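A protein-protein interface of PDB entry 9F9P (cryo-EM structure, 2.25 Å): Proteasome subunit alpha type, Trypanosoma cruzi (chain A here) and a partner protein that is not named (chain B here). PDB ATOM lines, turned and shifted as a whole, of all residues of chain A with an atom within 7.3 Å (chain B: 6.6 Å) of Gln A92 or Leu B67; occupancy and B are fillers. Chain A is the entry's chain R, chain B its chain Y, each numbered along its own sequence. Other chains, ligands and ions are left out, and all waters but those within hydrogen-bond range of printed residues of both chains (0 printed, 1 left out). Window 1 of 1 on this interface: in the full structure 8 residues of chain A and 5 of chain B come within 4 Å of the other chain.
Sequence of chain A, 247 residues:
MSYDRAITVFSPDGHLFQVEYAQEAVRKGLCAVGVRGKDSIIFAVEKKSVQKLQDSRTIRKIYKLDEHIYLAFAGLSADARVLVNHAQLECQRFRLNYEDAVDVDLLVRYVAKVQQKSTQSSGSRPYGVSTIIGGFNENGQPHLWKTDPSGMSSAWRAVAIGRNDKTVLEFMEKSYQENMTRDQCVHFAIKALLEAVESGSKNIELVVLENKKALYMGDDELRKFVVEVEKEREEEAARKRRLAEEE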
ATOM      1  N   LEU A  65     -27.495  -3.292  17.050  1.00  0.00           N
ATOM      2  CA  LEU A  65     -26.878  -3.658  18.321  1.00  0.00           C
ATOM      3  C   LEU A  65     -25.610  -2.850  18.569  1.00  0.00           C
ATOM      4  O   LEU A  65     -25.232  -2.627  19.697  1.00  0.00           O
ATOM      5  CB  LEU A  65     -26.596  -5.161  18.341  1.00  0.00           C
ATOM      6  CG  LEU A  65     -27.805  -6.067  18.073  1.00  0.00           C
ATOM      7  CD1 LEU A  65     -27.433  -7.555  18.001  1.00  0.00           C
ATOM      8  CD2 LEU A  65     -28.880  -5.858  19.151  1.00  0.00           C
ATOM      9  N   ASP A  66     -24.911  -2.479  17.503  1.00  0.00           N
ATOM     10  CA  ASP A  66     -23.718  -1.654  17.534  1.00  0.00           C
ATOM     11  C   ASP A  66     -23.614  -1.051  16.139  1.00  0.00           C
ATOM     12  O   ASP A  66     -24.492  -1.307  15.321  1.00  0.00           O
ATOM     13  CB  ASP A  66     -22.469  -2.452  17.953  1.00  0.00           C
ATOM     14  CG  ASP A  66     -21.323  -1.580  18.500  1.00  0.00           C
ATOM     15  OD1 ASP A  66     -21.362  -0.320  18.311  1.00  0.00           O
ATOM     16  OD2 ASP A  66     -20.374  -2.148  19.094  1.00  0.00           O
ATOM     17  N   GLU A  67     -22.575  -0.264  15.841  1.00  0.00           N
ATOM     18  CA  GLU A  67     -22.489   0.362  14.524  1.00  0.00           C
ATOM     19  C   GLU A  67     -22.493  -0.677  13.397  1.00  0.00           C
ATOM     20  O   GLU A  67     -23.037  -0.444  12.324  1.00  0.00           O
ATOM     21  CB  GLU A  67     -21.260   1.273  14.412  1.00  0.00           C
ATOM     22  CG  GLU A  67     -21.528   2.726  14.799  1.00  0.00           C
ATOM     23  CD  GLU A  67     -21.291   3.069  16.264  1.00  0.00           C
ATOM     24  OE1 GLU A  67     -20.123   2.947  16.721  1.00  0.00           O
ATOM     25  OE2 GLU A  67     -22.267   3.467  16.952  1.00  0.00           O
ATOM     26  N   ASN A  85     -31.874  -5.642  24.402  1.00  0.00           N
ATOM     27  CA  ASN A  85     -31.335  -4.758  25.408  1.00  0.00           C
ATOM     28  C   ASN A  85     -30.076  -5.355  26.020  1.00  0.00           C
ATOM     29  O   ASN A  85     -29.086  -4.643  26.106  1.00  0.00           O
ATOM     30  CB  ASN A  85     -32.384  -4.368  26.446  1.00  0.00           C
ATOM     31  CG  ASN A  85     -31.826  -3.377  27.444  1.00  0.00           C
ATOM     32  OD1 ASN A  85     -31.785  -2.174  27.172  1.00  0.00           O
ATOM     33  ND2 ASN A  85     -31.382  -3.867  28.595  1.00  0.00           N
ATOM     34  N   HIS A  86     -30.092  -6.643  26.406  1.00  0.00           N
ATOM     35  CA  HIS A  86     -28.906  -7.341  26.890  1.00  0.00           C
ATOM     36  C   HIS A  86     -27.761  -7.292  25.879  1.00  0.00           C
ATOM     37  O   HIS A  86     -26.609  -7.080  26.248  1.00  0.00           O
ATOM     38  CB  HIS A  86     -29.155  -8.823  27.205  1.00  0.00           C
ATOM     39  CG  HIS A  86     -29.976  -9.121  28.417  1.00  0.00           C
ATOM     40  ND1 HIS A  86     -29.638  -8.714  29.690  1.00  0.00           N
ATOM     41  CD2 HIS A  86     -31.119  -9.799  28.556  1.00  0.00           C
ATOM     42  CE1 HIS A  86     -30.563  -9.112  30.556  1.00  0.00           C
ATOM     43  NE2 HIS A  86     -31.478  -9.768  29.887  1.00  0.00           N
ATOM     44  N   ALA A  87     -28.030  -7.491  24.600  1.00  0.00           N
ATOM     45  CA  ALA A  87     -26.936  -7.508  23.655  1.00  0.00           C
ATOM     46  C   ALA A  87     -26.319  -6.119  23.401  1.00  0.00           C
ATOM     47  O   ALA A  87     -25.114  -5.994  23.159  1.00  0.00           O
ATOM     48  CB  ALA A  87     -27.407  -8.127  22.386  1.00  0.00           C
ATOM     49  N   GLN A  88     -27.120  -5.065  23.449  1.00  0.00           N
ATOM     50  CA  GLN A  88     -26.590  -3.715  23.394  1.00  0.00           C
ATOM     51  C   GLN A  88     -25.630  -3.417  24.549  1.00  0.00           C
ATOM     52  O   GLN A  88     -24.610  -2.793  24.295  1.00  0.00           O
ATOM     53  CB  GLN A  88     -27.743  -2.734  23.311  1.00  0.00           C
ATOM     54  CG  GLN A  88     -28.352  -2.677  21.904  1.00  0.00           C
ATOM     55  CD  GLN A  88     -29.618  -1.863  21.899  1.00  0.00           C
ATOM     56  OE1 GLN A  88     -30.165  -1.537  22.941  1.00  0.00           O
ATOM     57  NE2 GLN A  88     -30.130  -1.560  20.721  1.00  0.00           N
ATOM     58  N   LEU A  89     -25.937  -3.839  25.792  1.00  0.00           N
ATOM     59  CA  LEU A  89     -25.052  -3.608  26.919  1.00  0.00           C
ATOM     60  C   LEU A  89     -23.742  -4.377  26.778  1.00  0.00           C
ATOM     61  O   LEU A  89     -22.693  -3.828  27.088  1.00  0.00           O
ATOM     62  CB  LEU A  89     -25.718  -3.985  28.244  1.00  0.00           C
ATOM     63  CG  LEU A  89     -26.842  -3.060  28.717  1.00  0.00           C
ATOM     64  CD1 LEU A  89     -27.654  -3.718  29.827  1.00  0.00           C
ATOM     65  CD2 LEU A  89     -26.296  -1.734  29.212  1.00  0.00           C
ATOM     66  N   GLU A  90     -23.784  -5.622  26.304  1.00  0.00           N
ATOM     67  CA  GLU A  90     -22.591  -6.429  26.124  1.00  0.00           C
ATOM     68  C   GLU A  90     -21.656  -5.855  25.060  1.00  0.00           C
ATOM     69  O   GLU A  90     -20.442  -5.964  25.181  1.00  0.00           O
ATOM     70  CB  GLU A  90     -22.996  -7.844  25.726  1.00  0.00           C
ATOM     71  CG  GLU A  90     -21.837  -8.819  25.645  1.00  0.00           C
ATOM     72  CD  GLU A  90     -20.993  -9.037  26.911  1.00  0.00           C
ATOM     73  OE1 GLU A  90     -19.769  -9.243  26.756  1.00  0.00           O
ATOM     74  OE2 GLU A  90     -21.539  -8.999  28.058  1.00  0.00           O
ATOM     75  N   CYS A  91     -22.185  -5.305  23.981  1.00  0.00           N
ATOM     76  CA  CYS A  91     -21.330  -4.659  23.016  1.00  0.00           C
ATOM     77  C   CYS A  91     -20.550  -3.514  23.664  1.00  0.00           C
ATOM     78  O   CYS A  91     -19.367  -3.340  23.366  1.00  0.00           O
ATOM     79  CB  CYS A  91     -22.124  -4.151  21.818  1.00  0.00           C
ATOM     80  SG  CYS A  91     -22.642  -5.508  20.721  1.00  0.00           S
ATOM     81  N   GLN A  92     -21.164  -2.744  24.566  1.00  0.00           N
ATOM     82  CA  GLN A  92     -20.457  -1.609  25.148  1.00  0.00           C
ATOM     83  C   GLN A  92     -19.532  -2.083  26.258  1.00  0.00           C
ATOM     84  O   GLN A  92     -18.471  -1.524  26.449  1.00  0.00           O
ATOM     85  CB  GLN A  92     -21.398  -0.513  25.641  1.00  0.00           C
ATOM     86  CG  GLN A  92     -22.203   0.178  24.539  1.00  0.00           C
ATOM     87  CD  GLN A  92     -21.358   0.808  23.462  1.00  0.00           C
ATOM     88  OE1 GLN A  92     -20.357   1.465  23.727  1.00  0.00           O
ATOM     89  NE2 GLN A  92     -21.730   0.578  22.215  1.00  0.00           N
ATOM     90  N   ARG A  93     -19.914  -3.113  26.996  1.00  0.00           N
ATOM     91  CA  ARG A  93     -19.036  -3.676  28.008  1.00  0.00           C
ATOM     92  C   ARG A  93     -17.744  -4.196  27.365  1.00  0.00           C
ATOM     93  O   ARG A  93     -16.670  -4.095  27.932  1.00  0.00           O
ATOM     94  CB  ARG A  93     -19.804  -4.767  28.745  1.00  0.00           C
ATOM     95  CG  ARG A  93     -19.237  -5.140  30.103  1.00  0.00           C
ATOM     96  CD  ARG A  93     -19.673  -6.534  30.557  1.00  0.00           C
ATOM     97  NE  ARG A  93     -19.175  -7.606  29.687  1.00  0.00           N
ATOM     98  CZ  ARG A  93     -17.890  -7.937  29.522  1.00  0.00           C
ATOM     99  NH1 ARG A  93     -16.967  -7.451  30.338  1.00  0.00           N
ATOM    100  NH2 ARG A  93     -17.532  -8.779  28.562  1.00  0.00           N
ATOM    101  N   PHE A  94     -17.830  -4.720  26.158  1.00  0.00           N
ATOM    102  CA  PHE A  94     -16.667  -5.235  25.476  1.00  0.00           C
ATOM    103  C   PHE A  94     -15.700  -4.102  25.090  1.00  0.00           C
ATOM    104  O   PHE A  94     -14.507  -4.251  25.245  1.00  0.00           O
ATOM    105  CB  PHE A  94     -17.132  -6.065  24.270  1.00  0.00           C
ATOM    106  CG  PHE A  94     -16.031  -6.769  23.544  1.00  0.00           C
ATOM    107  CD1 PHE A  94     -15.818  -8.129  23.713  1.00  0.00           C
ATOM    108  CD2 PHE A  94     -15.185  -6.071  22.701  1.00  0.00           C
ATOM    109  CE1 PHE A  94     -14.796  -8.775  23.037  1.00  0.00           C
ATOM    110  CE2 PHE A  94     -14.165  -6.715  22.005  1.00  0.00           C
ATOM    111  CZ  PHE A  94     -13.976  -8.077  22.172  1.00  0.00           C
ATOM    112  N   ARG A  95     -16.188  -2.980  24.550  1.00  0.00           N
ATOM    113  CA  ARG A  95     -15.343  -1.823  24.265  1.00  0.00           C
ATOM    114  C   ARG A  95     -14.661  -1.272  25.508  1.00  0.00           C
ATOM    115  O   ARG A  95     -13.467  -0.993  25.478  1.00  0.00           O
ATOM    116  CB  ARG A  95     -16.142  -0.664  23.706  1.00  0.00           C
ATOM    117  CG  ARG A  95     -16.421  -0.802  22.219  1.00  0.00           C
ATOM    118  CD  ARG A  95     -17.381   0.301  21.844  1.00  0.00           C
ATOM    119  NE  ARG A  95     -17.976   0.059  20.540  1.00  0.00           N
ATOM    120  CZ  ARG A  95     -17.357   0.304  19.393  1.00  0.00           C
ATOM    121  NH1 ARG A  95     -17.961   0.021  18.253  1.00  0.00           N
ATOM    122  NH2 ARG A  95     -16.147   0.837  19.411  1.00  0.00           N
ATOM    123  N   LEU A  96     -15.382  -1.229  26.614  1.00  0.00           N
ATOM    124  CA  LEU A  96     -14.833  -0.763  27.867  1.00  0.00           C
ATOM    125  C   LEU A  96     -13.704  -1.663  28.363  1.00  0.00           C
ATOM    126  O   LEU A  96     -12.816  -1.192  29.055  1.00  0.00           O
ATOM    127  CB  LEU A  96     -15.966  -0.690  28.901  1.00  0.00           C
ATOM    128  CG  LEU A  96     -16.026   0.607  29.692  1.00  0.00           C
ATOM    129  CD1 LEU A  96     -15.966   1.797  28.759  1.00  0.00           C
ATOM    130  CD2 LEU A  96     -17.269   0.688  30.556  1.00  0.00           C
ATOM    131  N   ASN A  97     -13.735  -2.951  28.054  1.00  0.00           N
ATOM    132  CA  ASN A  97     -12.776  -3.886  28.609  1.00  0.00           C
ATOM    133  C   ASN A  97     -11.619  -4.205  27.682  1.00  0.00           C
ATOM    134  O   ASN A  97     -10.652  -4.821  28.124  1.00  0.00           O
ATOM    135  CB  ASN A  97     -13.375  -5.274  28.820  1.00  0.00           C
ATOM    136  CG  ASN A  97     -14.068  -5.422  30.150  1.00  0.00           C
ATOM    137  OD1 ASN A  97     -13.921  -6.460  30.790  1.00  0.00           O
ATOM    138  ND2 ASN A  97     -14.811  -4.398  30.562  1.00  0.00           N
ATOM    139  N   TYR A  98     -11.773  -3.997  26.381  1.00  0.00           N
ATOM    140  CA  TYR A  98     -10.801  -4.554  25.455  1.00  0.00           C
ATOM    141  C   TYR A  98     -10.436  -3.523  24.403  1.00  0.00           C
ATOM    142  O   TYR A  98      -9.580  -3.794  23.568  1.00  0.00           O
ATOM    143  CB  TYR A  98     -11.330  -5.826  24.793  1.00  0.00           C
ATOM    144  CG  TYR A  98     -11.641  -6.983  25.711  1.00  0.00           C
ATOM    145  CD1 TYR A  98     -10.635  -7.762  26.264  1.00  0.00           C
ATOM    146  CD2 TYR A  98     -12.950  -7.353  25.989  1.00  0.00           C
ATOM    147  CE1 TYR A  98     -10.918  -8.875  27.047  1.00  0.00           C
ATOM    148  CE2 TYR A  98     -13.252  -8.429  26.811  1.00  0.00           C
ATOM    149  CZ  TYR A  98     -12.233  -9.204  27.338  1.00  0.00           C
ATOM    150  OH  TYR A  98     -12.519 -10.292  28.129  1.00  0.00           O
ATOM    151  N   ASP A 100     -11.128  -2.653  21.511  1.00  0.00           N
ATOM    152  CA  ASP A 100     -11.590  -3.010  20.174  1.00  0.00           C
ATOM    153  C   ASP A 100     -13.131  -3.039  20.079  1.00  0.00           C
ATOM    154  O   ASP A 100     -13.831  -3.164  21.086  1.00  0.00           O
ATOM    155  CB  ASP A 100     -11.049  -4.398  19.797  1.00  0.00           C
ATOM    156  CG  ASP A 100      -9.532  -4.611  19.882  1.00  0.00           C
ATOM    157  OD1 ASP A 100      -9.091  -5.759  19.631  1.00  0.00           O
ATOM    158  OD2 ASP A 100      -8.792  -3.642  20.173  1.00  0.00           O
ATOM    159  N   VAL A 102     -16.459  -5.318  19.212  1.00  0.00           N
ATOM    160  CA  VAL A 102     -16.770  -6.734  19.350  1.00  0.00           C
ATOM    161  C   VAL A 102     -16.868  -7.407  17.976  1.00  0.00           C
ATOM    162  O   VAL A 102     -17.418  -6.845  17.050  1.00  0.00           O
ATOM    163  CB  VAL A 102     -18.067  -6.945  20.165  1.00  0.00           C
ATOM    164  CG1 VAL A 102     -19.323  -6.603  19.368  1.00  0.00           C
ATOM    165  CG2 VAL A 102     -18.191  -8.370  20.710  1.00  0.00           C
ATOM    166  N   LYS B  62     -18.417   8.104  26.861  1.00  0.00           N
ATOM    167  CA  LYS B  62     -18.622   7.722  25.465  1.00  0.00           C
ATOM    168  C   LYS B  62     -19.575   6.532  25.376  1.00  0.00           C
ATOM    169  O   LYS B  62     -20.413   6.487  24.492  1.00  0.00           O
ATOM    170  CB  LYS B  62     -17.310   7.310  24.789  1.00  0.00           C
ATOM    171  CG  LYS B  62     -16.663   8.340  23.906  1.00  0.00           C
ATOM    172  CD  LYS B  62     -15.183   8.064  23.595  1.00  0.00           C
ATOM    173  CE  LYS B  62     -14.934   7.155  22.411  1.00  0.00           C
ATOM    174  NZ  LYS B  62     -15.605   7.636  21.178  1.00  0.00           N
ATOM    175  N   CYS B  63     -19.397   5.550  26.253  1.00  0.00           N
ATOM    176  CA  CYS B  63     -20.235   4.361  26.275  1.00  0.00           C
ATOM    177  C   CYS B  63     -21.685   4.718  26.570  1.00  0.00           C
ATOM    178  O   CYS B  63     -22.568   4.272  25.861  1.00  0.00           O
ATOM    179  CB  CYS B  63     -19.732   3.323  27.281  1.00  0.00           C
ATOM    180  SG  CYS B  63     -21.021   2.332  28.111  1.00  0.00           S
ATOM    181  N   ASN B  64     -21.952   5.500  27.607  1.00  0.00           N
ATOM    182  CA  ASN B  64     -23.317   5.845  27.935  1.00  0.00           C
ATOM    183  C   ASN B  64     -23.961   6.686  26.838  1.00  0.00           C
ATOM    184  O   ASN B  64     -25.154   6.597  26.602  1.00  0.00           O
ATOM    185  CB  ASN B  64     -23.403   6.466  29.327  1.00  0.00           C
ATOM    186  CG  ASN B  64     -23.296   5.373  30.382  1.00  0.00           C
ATOM    187  OD1 ASN B  64     -24.294   4.742  30.745  1.00  0.00           O
ATOM    188  ND2 ASN B  64     -22.086   5.097  30.859  1.00  0.00           N
ATOM    189  N   MET B  65     -23.198   7.504  26.152  1.00  0.00           N
ATOM    190  CA  MET B  65     -23.765   8.296  25.086  1.00  0.00           C
ATOM    191  C   MET B  65     -24.107   7.453  23.863  1.00  0.00           C
ATOM    192  O   MET B  65     -25.041   7.801  23.153  1.00  0.00           O
ATOM    193  CB  MET B  65     -22.796   9.403  24.674  1.00  0.00           C
ATOM    194  CG  MET B  65     -23.018  10.663  25.524  1.00  0.00           C
ATOM    195  SD  MET B  65     -21.779  11.919  25.145  1.00  0.00           S
ATOM    196  CE  MET B  65     -22.332  12.404  23.507  1.00  0.00           C
ATOM    197  N   ALA B  66     -23.330   6.398  23.588  1.00  0.00           N
ATOM    198  CA  ALA B  66     -23.613   5.486  22.486  1.00  0.00           C
ATOM    199  C   ALA B  66     -24.849   4.632  22.783  1.00  0.00           C
ATOM    200  O   ALA B  66     -25.741   4.512  21.963  1.00  0.00           O
ATOM    201  CB  ALA B  66     -22.412   4.626  22.182  1.00  0.00           C
ATOM    202  N   LEU B  67     -24.966   4.144  23.994  1.00  0.00           N
ATOM    203  CA  LEU B  67     -26.160   3.431  24.411  1.00  0.00           C
ATOM    204  C   LEU B  67     -27.386   4.306  24.224  1.00  0.00           C
ATOM    205  O   LEU B  67     -28.301   3.929  23.539  1.00  0.00           O
ATOM    206  CB  LEU B  67     -25.976   3.074  25.888  1.00  0.00           C
ATOM    207  CG  LEU B  67     -26.324   1.664  26.333  1.00  0.00           C
ATOM    208  CD1 LEU B  67     -26.016   0.628  25.261  1.00  0.00           C
ATOM    209  CD2 LEU B  67     -25.533   1.353  27.588  1.00  0.00           C
ATOM    210  N   LYS B  68     -27.385   5.499  24.806  1.00  0.00           N
ATOM    211  CA  LYS B  68     -28.490   6.435  24.679  1.00  0.00           C
ATOM    212  C   LYS B  68     -28.810   6.754  23.232  1.00  0.00           C
ATOM    213  O   LYS B  68     -29.948   7.051  22.950  1.00  0.00           O
ATOM    214  CB  LYS B  68     -28.180   7.784  25.329  1.00  0.00           C
ATOM    215  CG  LYS B  68     -29.408   8.574  25.707  1.00  0.00           C
ATOM    216  CD  LYS B  68     -29.203  10.048  25.899  1.00  0.00           C
ATOM    217  CE  LYS B  68     -30.535  10.729  26.151  1.00  0.00           C
ATOM    218  NZ  LYS B  68     -30.401  12.202  26.269  1.00  0.00           N
ATOM    219  N   ARG B  69     -27.827   6.712  22.341  1.00  0.00           N
ATOM    220  CA  ARG B  69     -28.061   7.044  20.947  1.00  0.00           C
ATOM    221  C   ARG B  69     -28.961   5.982  20.336  1.00  0.00           C
ATOM    222  O   ARG B  69     -29.953   6.359  19.731  1.00  0.00           O
ATOM    223  CB  ARG B  69     -26.762   7.146  20.133  1.00  0.00           C
ATOM    224  CG  ARG B  69     -26.635   8.410  19.295  1.00  0.00           C
ATOM    225  CD  ARG B  69     -25.602   8.363  18.178  1.00  0.00           C
ATOM    226  NE  ARG B  69     -24.346   7.664  18.467  1.00  0.00           N
ATOM    227  CZ  ARG B  69     -23.376   8.088  19.288  1.00  0.00           C
ATOM    228  NH1 ARG B  69     -22.244   7.411  19.373  1.00  0.00           N
ATOM    229  NH2 ARG B  69     -23.519   9.187  20.012  1.00  0.00           N
ATOM    230  N   MET B  70     -28.629   4.682  20.489  1.00  0.00           N
ATOM    231  CA  MET B  70     -29.373   3.624  19.800  1.00  0.00           C
ATOM    232  C   MET B  70     -30.738   3.332  20.424  1.00  0.00           C
ATOM    233  O   MET B  70     -31.620   2.831  19.738  1.00  0.00           O
ATOM    234  CB  MET B  70     -28.638   2.293  19.648  1.00  0.00           C
ATOM    235  CG  MET B  70     -27.745   1.946  20.760  1.00  0.00           C
ATOM    236  SD  MET B  70     -26.733   0.589  20.222  1.00  0.00           S
ATOM    237  CE  MET B  70     -25.622   1.439  19.085  1.00  0.00           C
ATOM    238  N   ARG B  71     -30.967   3.690  21.672  1.00  0.00           N
ATOM    239  CA  ARG B  71     -32.320   3.665  22.197  1.00  0.00           C
ATOM    240  C   ARG B  71     -32.984   5.016  21.943  1.00  0.00           C
ATOM    241  O   ARG B  71     -33.625   5.569  22.839  1.00  0.00           O
ATOM    242  CB  ARG B  71     -32.275   3.346  23.695  1.00  0.00           C
ATOM    243  CG  ARG B  71     -31.402   2.144  24.022  1.00  0.00           C
ATOM    244  CD  ARG B  71     -31.769   1.539  25.358  1.00  0.00           C
ATOM    245  NE  ARG B  71     -30.822   1.794  26.434  1.00  0.00           N
ATOM    246  CZ  ARG B  71     -30.071   0.855  27.000  1.00  0.00           C
ATOM    247  NH1 ARG B  71     -29.398   1.131  28.103  1.00  0.00           N
ATOM    248  NH2 ARG B  71     -30.030  -0.365  26.483  1.00  0.00           N
ATOM    249  N   GLU B  72     -32.806   5.555  20.729  1.00  0.00           N
ATOM    250  CA  GLU B  72     -33.349   6.868  20.386  1.00  0.00           C
ATOM    251  C   GLU B  72     -33.208   7.150  18.884  1.00  0.00           C
ATOM    252  O   GLU B  72     -33.212   8.311  18.473  1.00  0.00           O
ATOM    253  CB  GLU B  72     -32.666   7.955  21.225  1.00  0.00           C
ATOM    254  CG  GLU B  72     -33.547   9.151  21.537  1.00  0.00           C
ATOM    255  CD  GLU B  72     -33.209   9.897  22.826  1.00  0.00           C
ATOM    256  OE1 GLU B  72     -33.698  11.040  22.995  1.00  0.00           O
ATOM    257  OE2 GLU B  72     -32.487   9.336  23.674  1.00  0.00           O
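NH2 of Arg B71 lies within hydrogen-bond range of OD1 of Asn A85 (2.6 Å). The side-chain sulfur of Met B70 sits close to the backbone carbonyl oxygen of Leu A65, at 3.6 Å.
OD2 of Asp A66 lies within salt-bridge range of NH1 of Arg A95 (3.4 Å).
Asp A66 touches Met B70 (CA to CE, 3.9 Å). Leu B67 touches Gln A88. Gln A88 touches Arg B71 (OE1 to NH2, 3.7 Å). CD2 of Leu A89 touches CD2 of Leu B67, 3.6 Å away. Gln A92 touches Cys B63 (CB to SG, 3.8 Å). CD1 of Leu B67 touches CG of Gln A92, 3.9 Å away.
Leu B67 touches three residues of chain A. Ala B66 touches none of the printed residues of chain A. Printed residues of chain B within 4 Å of Asp A66: Met B70. Printed residues of chain B within 4 Å of Leu A65: Met B70. Of the printed residues of chain B, Gln A88 touches Leu B67 and Arg B71. Printed residues of chain A within 4 Å of Cys B63: Gln A92 (3.8 Å). Leu A96 touches none of the printed residues of chain B. The nearest residue of chain A that does not touch Leu B67 is Asn A85 (6.2 Å). The nearest printed residue of chain B that does not touch Asp A66 is Ala B66 (6.4 Å).
Of the 11 printed residues of chain B, 4 touch a printed residue of chain A. Along chain B the printed residues that touch a printed residue of chain A span positions 63 to 71. Of the 19 printed residues of chain A, 6 touch a printed residue of chain B. Along chain A the printed residues that touch a printed residue of chain B span positions 65 to 92. Among the printed residues, 8 pairs touch across the chains. Among the printed residues, no Asp or Glu carboxylate lies within 4 Å of a Lys or Arg side-chain nitrogen of the other chain.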
